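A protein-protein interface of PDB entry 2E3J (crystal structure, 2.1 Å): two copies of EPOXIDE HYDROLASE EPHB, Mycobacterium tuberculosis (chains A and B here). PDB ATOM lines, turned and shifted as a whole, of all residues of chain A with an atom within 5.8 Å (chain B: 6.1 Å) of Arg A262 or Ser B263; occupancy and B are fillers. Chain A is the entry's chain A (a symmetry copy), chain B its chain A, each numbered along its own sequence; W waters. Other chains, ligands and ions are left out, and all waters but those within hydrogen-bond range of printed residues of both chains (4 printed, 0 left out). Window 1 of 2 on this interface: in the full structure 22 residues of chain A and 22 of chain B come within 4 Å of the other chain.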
ATOM      1  N   GLY A  66      17.014 -20.695  17.974  1.00  0.00           N
ATOM      2  CA  GLY A  66      18.103 -19.880  18.490  1.00  0.00           C
ATOM      3  C   GLY A  66      18.636 -20.179  19.869  1.00  0.00           C
ATOM      4  O   GLY A  66      19.296 -21.193  20.069  1.00  0.00           O
ATOM      5  N   LYS A  70      14.888 -25.691  24.240  1.00  0.00           N
ATOM      6  CA  LYS A  70      14.754 -26.741  23.222  1.00  0.00           C
ATOM      7  C   LYS A  70      14.142 -27.999  23.835  1.00  0.00           C
ATOM      8  O   LYS A  70      14.791 -28.703  24.605  1.00  0.00           O
ATOM      9  CB  LYS A  70      16.127 -27.106  22.636  1.00  0.00           C
ATOM     10  CG  LYS A  70      16.955 -25.934  22.110  1.00  0.00           C
ATOM     11  CD  LYS A  70      16.339 -25.290  20.891  1.00  0.00           C
ATOM     12  CE  LYS A  70      17.319 -24.325  20.219  1.00  0.00           C
ATOM     13  NZ  LYS A  70      17.946 -23.399  21.184  1.00  0.00           N
ATOM     14  N   THR A 257      22.643 -19.833   9.097  1.00  0.00           N
ATOM     15  CA  THR A 257      23.377 -21.094   9.097  1.00  0.00           C
ATOM     16  C   THR A 257      23.946 -21.350  10.482  1.00  0.00           C
ATOM     17  O   THR A 257      23.866 -22.463  11.006  1.00  0.00           O
ATOM     18  CB  THR A 257      24.545 -21.089   8.076  1.00  0.00           C
ATOM     19  OG1 THR A 257      24.019 -21.040   6.743  1.00  0.00           O
ATOM     20  CG2 THR A 257      25.398 -22.365   8.229  1.00  0.00           C
ATOM     21  N   GLY A 258      24.517 -20.310  11.077  1.00  0.00           N
ATOM     22  CA  GLY A 258      25.086 -20.442  12.406  1.00  0.00           C
ATOM     23  C   GLY A 258      24.070 -20.753  13.497  1.00  0.00           C
ATOM     24  O   GLY A 258      24.375 -21.487  14.434  1.00  0.00           O
ATOM     25  N   GLU A 259      22.865 -20.198  13.391  1.00  0.00           N
ATOM     26  CA  GLU A 259      21.833 -20.448  14.403  1.00  0.00           C
ATOM     27  C   GLU A 259      21.367 -21.898  14.358  1.00  0.00           C
ATOM     28  O   GLU A 259      21.247 -22.567  15.392  1.00  0.00           O
ATOM     29  CB  GLU A 259      20.612 -19.547  14.177  1.00  0.00           C
ATOM     30  CG  GLU A 259      20.874 -18.065  14.335  1.00  0.00           C
ATOM     31  CD  GLU A 259      21.337 -17.707  15.724  1.00  0.00           C
ATOM     32  OE1 GLU A 259      20.518 -17.776  16.668  1.00  0.00           O
ATOM     33  OE2 GLU A 259      22.528 -17.361  15.877  1.00  0.00           O
ATOM     34  N   PHE A 260      21.100 -22.377  13.151  1.00  0.00           N
ATOM     35  CA  PHE A 260      20.612 -23.738  12.987  1.00  0.00           C
ATOM     36  C   PHE A 260      21.650 -24.835  13.111  1.00  0.00           C
ATOM     37  O   PHE A 260      21.308 -25.955  13.501  1.00  0.00           O
ATOM     38  CB  PHE A 260      19.821 -23.852  11.675  1.00  0.00           C
ATOM     39  CG  PHE A 260      18.494 -23.160  11.730  1.00  0.00           C
ATOM     40  CD1 PHE A 260      17.429 -23.733  12.424  1.00  0.00           C
ATOM     41  CD2 PHE A 260      18.329 -21.900  11.174  1.00  0.00           C
ATOM     42  CE1 PHE A 260      16.226 -23.056  12.564  1.00  0.00           C
ATOM     43  CE2 PHE A 260      17.125 -21.210  11.312  1.00  0.00           C
ATOM     44  CZ  PHE A 260      16.071 -21.784  12.007  1.00  0.00           C
ATOM     45  N   GLU A 261      22.914 -24.565  12.812  1.00  0.00           N
ATOM     46  CA  GLU A 261      23.853 -25.661  13.000  1.00  0.00           C
ATOM     47  C   GLU A 261      24.018 -25.875  14.500  1.00  0.00           C
ATOM     48  O   GLU A 261      24.501 -26.907  14.946  1.00  0.00           O
ATOM     49  CB  GLU A 261      25.201 -25.426  12.289  1.00  0.00           C
ATOM     50  CG  GLU A 261      25.980 -24.182  12.631  1.00  0.00           C
ATOM     51  CD  GLU A 261      27.323 -24.155  11.899  1.00  0.00           C
ATOM     52  OE1 GLU A 261      27.354 -24.487  10.694  1.00  0.00           O
ATOM     53  OE2 GLU A 261      28.342 -23.808  12.525  1.00  0.00           O
ATOM     54  N   ARG A 262      23.565 -24.901  15.283  1.00  0.00           N
ATOM     55  CA  ARG A 262      23.632 -25.012  16.732  1.00  0.00           C
ATOM     56  C   ARG A 262      22.320 -25.527  17.333  1.00  0.00           C
ATOM     57  O   ARG A 262      22.332 -26.299  18.287  1.00  0.00           O
ATOM     58  CB  ARG A 262      23.990 -23.668  17.354  1.00  0.00           C
ATOM     59  CG  ARG A 262      25.442 -23.272  17.157  1.00  0.00           C
ATOM     60  CD  ARG A 262      25.711 -21.921  17.794  1.00  0.00           C
ATOM     61  NE  ARG A 262      27.127 -21.565  17.763  1.00  0.00           N
ATOM     62  CZ  ARG A 262      28.035 -21.988  18.640  1.00  0.00           C
ATOM     63  NH1 ARG A 262      27.689 -22.791  19.642  1.00  0.00           N
ATOM     64  NH2 ARG A 262      29.302 -21.607  18.511  1.00  0.00           N
ATOM     65  N   SER A 263      21.193 -25.124  16.757  1.00  0.00           N
ATOM     66  CA  SER A 263      19.892 -25.539  17.281  1.00  0.00           C
ATOM     67  C   SER A 263      19.308 -26.795  16.644  1.00  0.00           C
ATOM     68  O   SER A 263      18.617 -27.574  17.312  1.00  0.00           O
ATOM     69  CB  SER A 263      18.877 -24.414  17.115  1.00  0.00           C
ATOM     70  OG  SER A 263      18.524 -24.263  15.748  1.00  0.00           O
ATOM     71  N   GLY A 264      19.578 -26.990  15.361  1.00  0.00           N
ATOM     72  CA  GLY A 264      19.018 -28.131  14.666  1.00  0.00           C
ATOM     73  C   GLY A 264      17.616 -27.767  14.203  1.00  0.00           C
ATOM     74  O   GLY A 264      17.171 -26.626  14.378  1.00  0.00           O
ATOM     75  N   ARG B  14      27.590 -33.418   9.667  1.00  0.00           N
ATOM     76  CA  ARG B  14      28.443 -32.253   9.875  1.00  0.00           C
ATOM     77  C   ARG B  14      29.056 -32.353  11.254  1.00  0.00           C
ATOM     78  O   ARG B  14      28.341 -32.406  12.252  1.00  0.00           O
ATOM     79  CB  ARG B  14      27.634 -30.948   9.778  1.00  0.00           C
ATOM     80  CG  ARG B  14      28.502 -29.690   9.811  1.00  0.00           C
ATOM     81  CD  ARG B  14      27.691 -28.407   9.927  1.00  0.00           C
ATOM     82  NE  ARG B  14      26.924 -28.351  11.170  1.00  0.00           N
ATOM     83  CZ  ARG B  14      25.631 -28.650  11.273  1.00  0.00           C
ATOM     84  NH1 ARG B  14      24.951 -29.027  10.204  1.00  0.00           N
ATOM     85  NH2 ARG B  14      25.017 -28.558  12.451  1.00  0.00           N
ATOM     86  N   GLY B  64      24.904 -33.954  17.850  1.00  0.00           N
ATOM     87  CA  GLY B  64      23.931 -33.559  18.857  1.00  0.00           C
ATOM     88  C   GLY B  64      24.451 -32.451  19.760  1.00  0.00           C
ATOM     89  O   GLY B  64      23.704 -31.869  20.549  1.00  0.00           O
ATOM     90  N   TYR B  65      25.740 -32.146  19.635  1.00  0.00           N
ATOM     91  CA  TYR B  65      26.383 -31.124  20.459  1.00  0.00           C
ATOM     92  C   TYR B  65      26.934 -29.920  19.685  1.00  0.00           C
ATOM     93  O   TYR B  65      27.227 -29.996  18.492  1.00  0.00           O
ATOM     94  CB  TYR B  65      27.549 -31.751  21.245  1.00  0.00           C
ATOM     95  CG  TYR B  65      27.189 -32.635  22.418  1.00  0.00           C
ATOM     96  CD1 TYR B  65      27.246 -32.141  23.726  1.00  0.00           C
ATOM     97  CD2 TYR B  65      26.914 -34.000  22.238  1.00  0.00           C
ATOM     98  CE1 TYR B  65      27.063 -32.981  24.830  1.00  0.00           C
ATOM     99  CE2 TYR B  65      26.722 -34.849  23.333  1.00  0.00           C
ATOM    100  CZ  TYR B  65      26.804 -34.334  24.630  1.00  0.00           C
ATOM    101  OH  TYR B  65      26.651 -35.168  25.728  1.00  0.00           O
ATOM    102  N   GLY B  66      27.084 -28.808  20.401  1.00  0.00           N
ATOM    103  CA  GLY B  66      27.643 -27.593  19.829  1.00  0.00           C
ATOM    104  C   GLY B  66      27.205 -27.179  18.447  1.00  0.00           C
ATOM    105  O   GLY B  66      26.071 -26.747  18.263  1.00  0.00           O
ATOM    106  N   ARG B  67      28.106 -27.284  17.471  1.00  0.00           N
ATOM    107  CA  ARG B  67      27.777 -26.896  16.106  1.00  0.00           C
ATOM    108  C   ARG B  67      27.689 -28.108  15.171  1.00  0.00           C
ATOM    109  O   ARG B  67      27.606 -27.954  13.947  1.00  0.00           O
ATOM    110  CB  ARG B  67      28.816 -25.890  15.579  1.00  0.00           C
ATOM    111  CG  ARG B  67      28.823 -24.547  16.322  1.00  0.00           C
ATOM    112  CD  ARG B  67      30.004 -23.689  15.891  1.00  0.00           C
ATOM    113  NE  ARG B  67      30.069 -23.570  14.435  1.00  0.00           N
ATOM    114  CZ  ARG B  67      31.068 -22.996  13.766  1.00  0.00           C
ATOM    115  NH1 ARG B  67      32.106 -22.475  14.420  1.00  0.00           N
ATOM    116  NH2 ARG B  67      31.034 -22.952  12.441  1.00  0.00           N
ATOM    117  N   SER B  68      27.706 -29.310  15.743  1.00  0.00           N
ATOM    118  CA  SER B  68      27.611 -30.519  14.928  1.00  0.00           C
ATOM    119  C   SER B  68      26.157 -30.884  14.660  1.00  0.00           C
ATOM    120  O   SER B  68      25.255 -30.429  15.367  1.00  0.00           O
ATOM    121  CB  SER B  68      28.323 -31.669  15.613  1.00  0.00           C
ATOM    122  OG  SER B  68      29.709 -31.380  15.711  1.00  0.00           O
ATOM    123  N   LYS B  70      22.465 -32.117  14.364  1.00  0.00           N
ATOM    124  CA  LYS B  70      21.492 -32.428  15.418  1.00  0.00           C
ATOM    125  C   LYS B  70      20.370 -33.304  14.864  1.00  0.00           C
ATOM    126  O   LYS B  70      19.528 -32.839  14.101  1.00  0.00           O
ATOM    127  CB  LYS B  70      20.869 -31.140  15.979  1.00  0.00           C
ATOM    128  CG  LYS B  70      21.859 -30.073  16.444  1.00  0.00           C
ATOM    129  CD  LYS B  70      22.649 -30.504  17.657  1.00  0.00           C
ATOM    130  CE  LYS B  70      23.409 -29.326  18.270  1.00  0.00           C
ATOM    131  NZ  LYS B  70      24.160 -28.555  17.259  1.00  0.00           N
ATOM    132  N   GLY B 258      26.105 -21.161  27.077  1.00  0.00           N
ATOM    133  CA  GLY B 258      25.824 -20.675  25.738  1.00  0.00           C
ATOM    134  C   GLY B 258      25.699 -21.769  24.686  1.00  0.00           C
ATOM    135  O   GLY B 258      24.894 -21.652  23.767  1.00  0.00           O
ATOM    136  N   GLU B 259      26.492 -22.831  24.806  1.00  0.00           N
ATOM    137  CA  GLU B 259      26.432 -23.925  23.832  1.00  0.00           C
ATOM    138  C   GLU B 259      25.111 -24.676  23.937  1.00  0.00           C
ATOM    139  O   GLU B 259      24.453 -24.964  22.930  1.00  0.00           O
ATOM    140  CB  GLU B 259      27.570 -24.928  24.060  1.00  0.00           C
ATOM    141  CG  GLU B 259      28.963 -24.375  23.847  1.00  0.00           C
ATOM    142  CD  GLU B 259      29.180 -23.893  22.434  1.00  0.00           C
ATOM    143  OE1 GLU B 259      29.255 -24.741  21.516  1.00  0.00           O
ATOM    144  OE2 GLU B 259      29.270 -22.663  22.239  1.00  0.00           O
ATOM    145  N   PHE B 260      24.729 -24.995  25.166  1.00  0.00           N
ATOM    146  CA  PHE B 260      23.502 -25.745  25.388  1.00  0.00           C
ATOM    147  C   PHE B 260      22.212 -24.958  25.272  1.00  0.00           C
ATOM    148  O   PHE B 260      21.177 -25.534  24.930  1.00  0.00           O
ATOM    149  CB  PHE B 260      23.588 -26.499  26.723  1.00  0.00           C
ATOM    150  CG  PHE B 260      24.536 -27.657  26.681  1.00  0.00           C
ATOM    151  CD1 PHE B 260      24.176 -28.840  26.036  1.00  0.00           C
ATOM    152  CD2 PHE B 260      25.817 -27.543  27.199  1.00  0.00           C
ATOM    153  CE1 PHE B 260      25.081 -29.882  25.906  1.00  0.00           C
ATOM    154  CE2 PHE B 260      26.737 -28.585  27.071  1.00  0.00           C
ATOM    155  CZ  PHE B 260      26.373 -29.756  26.424  1.00  0.00           C
ATOM    156  N   GLU B 261      22.225 -23.656  25.528  1.00  0.00           N
ATOM    157  CA  GLU B 261      20.956 -22.968  25.352  1.00  0.00           C
ATOM    158  C   GLU B 261      20.672 -22.900  23.855  1.00  0.00           C
ATOM    159  O   GLU B 261      19.550 -22.652  23.431  1.00  0.00           O
ATOM    160  CB  GLU B 261      20.927 -21.578  26.018  1.00  0.00           C
ATOM    161  CG  GLU B 261      21.975 -20.572  25.614  1.00  0.00           C
ATOM    162  CD  GLU B 261      21.746 -19.229  26.308  1.00  0.00           C
ATOM    163  OE1 GLU B 261      21.447 -19.226  27.522  1.00  0.00           O
ATOM    164  OE2 GLU B 261      21.859 -18.182  25.644  1.00  0.00           O
ATOM    165  N   ARG B 262      21.697 -23.170  23.053  1.00  0.00           N
ATOM    166  CA  ARG B 262      21.535 -23.175  21.607  1.00  0.00           C
ATOM    167  C   ARG B 262      21.285 -24.584  21.060  1.00  0.00           C
ATOM    168  O   ARG B 262      20.501 -24.761  20.131  1.00  0.00           O
ATOM    169  CB  ARG B 262      22.760 -22.570  20.931  1.00  0.00           C
ATOM    170  CG  ARG B 262      22.855 -21.062  21.076  1.00  0.00           C
ATOM    171  CD  ARG B 262      24.104 -20.544  20.388  1.00  0.00           C
ATOM    172  NE  ARG B 262      24.162 -19.086  20.369  1.00  0.00           N
ATOM    173  CZ  ARG B 262      23.539 -18.312  19.482  1.00  0.00           C
ATOM    174  NH1 ARG B 262      22.798 -18.848  18.518  1.00  0.00           N
ATOM    175  NH2 ARG B 262      23.655 -16.991  19.564  1.00  0.00           N
ATOM    176  N   SER B 263      21.925 -25.585  21.651  1.00  0.00           N
ATOM    177  CA  SER B 263      21.773 -26.959  21.177  1.00  0.00           C
ATOM    178  C   SER B 263      20.681 -27.767  21.871  1.00  0.00           C
ATOM    179  O   SER B 263      20.043 -28.623  21.247  1.00  0.00           O
ATOM    180  CB  SER B 263      23.086 -27.718  21.333  1.00  0.00           C
ATOM    181  OG  SER B 263      23.343 -27.986  22.702  1.00  0.00           O
ATOM    182  N   GLY B 264      20.470 -27.500  23.151  1.00  0.00           N
ATOM    183  CA  GLY B 264      19.487 -28.258  23.898  1.00  0.00           C
ATOM    184  C   GLY B 264      20.143 -29.540  24.387  1.00  0.00           C
ATOM    185  O   GLY B 264      21.345 -29.747  24.186  1.00  0.00           O
ATOM    186  N   PHE B 265      19.371 -30.408  25.028  1.00  0.00           N
ATOM    187  CA  PHE B 265      19.929 -31.655  25.529  1.00  0.00           C
ATOM    188  C   PHE B 265      19.361 -32.879  24.830  1.00  0.00           C
ATOM    189  O   PHE B 265      19.744 -33.996  25.140  1.00  0.00           O
ATOM    190  CB  PHE B 265      19.703 -31.761  27.035  1.00  0.00           C
ATOM    191  CG  PHE B 265      20.544 -30.802  27.839  1.00  0.00           C
ATOM    192  CD1 PHE B 265      21.643 -31.251  28.549  1.00  0.00           C
ATOM    193  CD2 PHE B 265      20.235 -29.449  27.877  1.00  0.00           C
ATOM    194  CE1 PHE B 265      22.429 -30.365  29.290  1.00  0.00           C
ATOM    195  CE2 PHE B 265      21.010 -28.559  28.612  1.00  0.00           C
ATOM    196  CZ  PHE B 265      22.108 -29.019  29.320  1.00  0.00           C
ATOM    197  N   GLY B 266      18.461 -32.657  23.878  1.00  0.00           N
ATOM    198  CA  GLY B 266      17.851 -33.754  23.147  1.00  0.00           C
ATOM    199  C   GLY B 266      18.841 -34.755  22.582  1.00  0.00           C
ATOM    200  O   GLY B 266      18.823 -35.923  22.957  1.00  0.00           O
ATOM    201  N   GLY B 267      19.704 -34.302  21.677  1.00  0.00           N
ATOM    202  CA  GLY B 267      20.695 -35.185  21.079  1.00  0.00           C
ATOM    203  C   GLY B 267      21.574 -35.836  22.128  1.00  0.00           C
ATOM    204  O   GLY B 267      21.770 -37.050  22.108  1.00  0.00           O
ATOM    205  N   PRO B 268      22.142 -35.043  23.052  1.00  0.00           N
ATOM    206  CA  PRO B 268      22.999 -35.562  24.113  1.00  0.00           C
ATOM    207  C   PRO B 268      22.346 -36.690  24.927  1.00  0.00           C
ATOM    208  O   PRO B 268      22.960 -37.743  25.151  1.00  0.00           O
ATOM    209  CB  PRO B 268      23.262 -34.328  24.965  1.00  0.00           C
ATOM    210  CG  PRO B 268      23.322 -33.237  23.939  1.00  0.00           C
ATOM    211  CD  PRO B 268      22.154 -33.566  23.043  1.00  0.00           C
HETATM  212  O   HOH W   1      20.984 -21.408  17.970  1.00  0.00           O
HETATM  213  O   HOH W   2      22.103 -28.586  12.981  1.00  0.00           O
HETATM  214  O   HOH W   3      16.981 -29.275  25.843  1.00  0.00           O
HETATM  215  O   HOH W   4      25.571 -25.070  20.322  1.00  0.00           O
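Gly A66 touches Arg B262, and with the chains exchanged Arg A262 touches Gly B66. Lys A70 touches Glu B261, and with the chains exchanged Glu A261 touches Lys B70. Lys A70 touches Arg B262, and with the chains exchanged Arg A262 touches Lys B70. Glu A259 touches Arg B262, and with the chains exchanged Arg A262 touches Glu B259. Positions printed for both chains: 66, 70, 258, 259, 260, 261, 262, 263 and 264. Of the 19 pairs that touch across the chains among the printed residues, 15 have their exchanged pair printed and touching as well.
Printed residues of chain B within 4 Å of Gly A66: Glu B261 (3.7 Å) and Arg B262 (3.4 Å). Of the printed residues of chain B, Glu A261 touches Arg B14 (3.0 Å), Gly B66 (3.7 Å), Arg B67 (2.6 Å), Ser B68 (3.6 Å) and Lys B70 (2.9 Å). Arg A262 touches just these residues of chain B: Gly B66 (3.4 Å), Arg B67 (3.4 Å), Lys B70 (3.1 Å), Glu B259 (3.0 Å), Arg B262 (3.0 Å) and Ser B263 (3.0 Å). Of the printed residues of chain B, Gly A264 touches Lys B70. Of the printed residues of chain A, Arg B14 touches Glu A261 (3.0 Å). Printed residues of chain A within 4 Å of Gly B66: Glu A261 and Arg A262. Ser B263 touches just one residue of chain A: Arg A262 (3.0 Å). Gly B266 touches none of the printed residues of chain A. The nearest residue of chain B that does not touch Arg A262 is Arg B14 (4.8 Å). The nearest residue of chain A that does not touch Ser B263 is Lys A70 (4.2 Å).
O of Ser B68 sits close to NH2 of Arg B14. O of Gly B66 sits at hydrogen-bond distance from NZ of Lys B70 (2.8 Å). The backbone carbonyl oxygen (O) of Ser B68 sits at hydrogen-bond distance from the side-chain amino group (NZ) of Lys B70 (2.9 Å). O of Glu B259 lies within hydrogen-bond range of OG of Ser B263 (3.2 Å). The backbone carbonyl oxygen (O) of Gly A66 lies within hydrogen-bond range of the side-chain amino group (NZ) of Lys A70 (2.8 Å). O of Glu A259 sits at hydrogen-bond distance from OG of Ser A263, 3.2 Å away.
The side-chain carboxylate (OE1) of Glu A261 lies within salt-bridge range of the guanidinium group (NE) of Arg B14 (3.9 Å). OE2 of Glu A261 is in salt-bridge range of NE of Arg B67, 2.6 Å away. The side-chain amino group of Lys B70 lies within hydrogen-bond range of the backbone carbonyl oxygen of Glu A261, 2.9 Å away. The backbone carbonyl oxygen (O) of Arg A262 lies within hydrogen-bond range of the side-chain amino group (NZ) of Lys B70, 3.1 Å away. The side-chain carboxylate (OE2) of Glu B259 is in salt-bridge range of the guanidinium group (NH1) of Arg A262, at 3.0 Å. O of Glu B261 is in hydrogen-bond range of NZ of Lys A70 (2.9 Å). The side-chain amino group (NZ) of Lys A70 sits at hydrogen-bond distance from the backbone carbonyl oxygen (O) of Arg B262 (3.1 Å). The side-chain carboxylate (OE2) of Glu A259 is in salt-bridge range of the guanidinium group (NH1) of Arg B262, at 3.0 Å. The backbone carbonyl oxygen (O) of Arg B262 sits close to the backbone NH (N) of Ser A263 (3.5 Å). The backbone carbonyl oxygen of Arg A262 lies close to the backbone NH of Ser B263, at 3.5 Å. O of Arg A262 sits close to O of Arg B262, at 3.0 Å.
Water W3 bridges the backbone carbonyl oxygen of Lys A70 and the backbone NH of Phe B265. Water W4 lies within hydrogen-bond range of the backbone carbonyl oxygen of Gly B66, the backbone carbonyl oxygen of Glu B259 and the guanidinium group of Arg A262. Water W1 lies within hydrogen-bond range of O of Gly A66, O of Glu A259 and NH1 of Arg B262. Water W2 bridges the backbone carbonyl oxygen of Phe A260 (2.8 Å) and the guanidinium group of Arg B14 (3.0 Å).
Among the printed residues, merely in contact across the chains: Gly A66 with Glu B261, Gly A66 with Arg B262, Lys A70 with Gly B264, Glu A261 with Gly B66, Glu A261 with Ser B68, Arg A262 with Gly B66, Arg A262 with Arg B67 and Gly A264 with Lys B70.
Of the 10 printed residues of chain A, 7 touch a printed residue of chain B. Printed residues of chain A that touch a printed residue of chain B: Gly A66, Lys A70, Glu A259, Glu A261, Arg A262, Ser A263 and Gly A264. Of the 18 printed residues of chain B, 10 touch a printed residue of chain A. Among the printed residues, Asp or Glu carboxylates within 4 Å of a Lys or Arg side-chain nitrogen of the other chain: Glu A259 with Arg B262 (3.0 Å), Glu A261 with Arg B14 (3.9 Å), Glu A261 with Arg B67 (2.6 Å) and Arg A262 with Glu B259 (3.0 Å).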
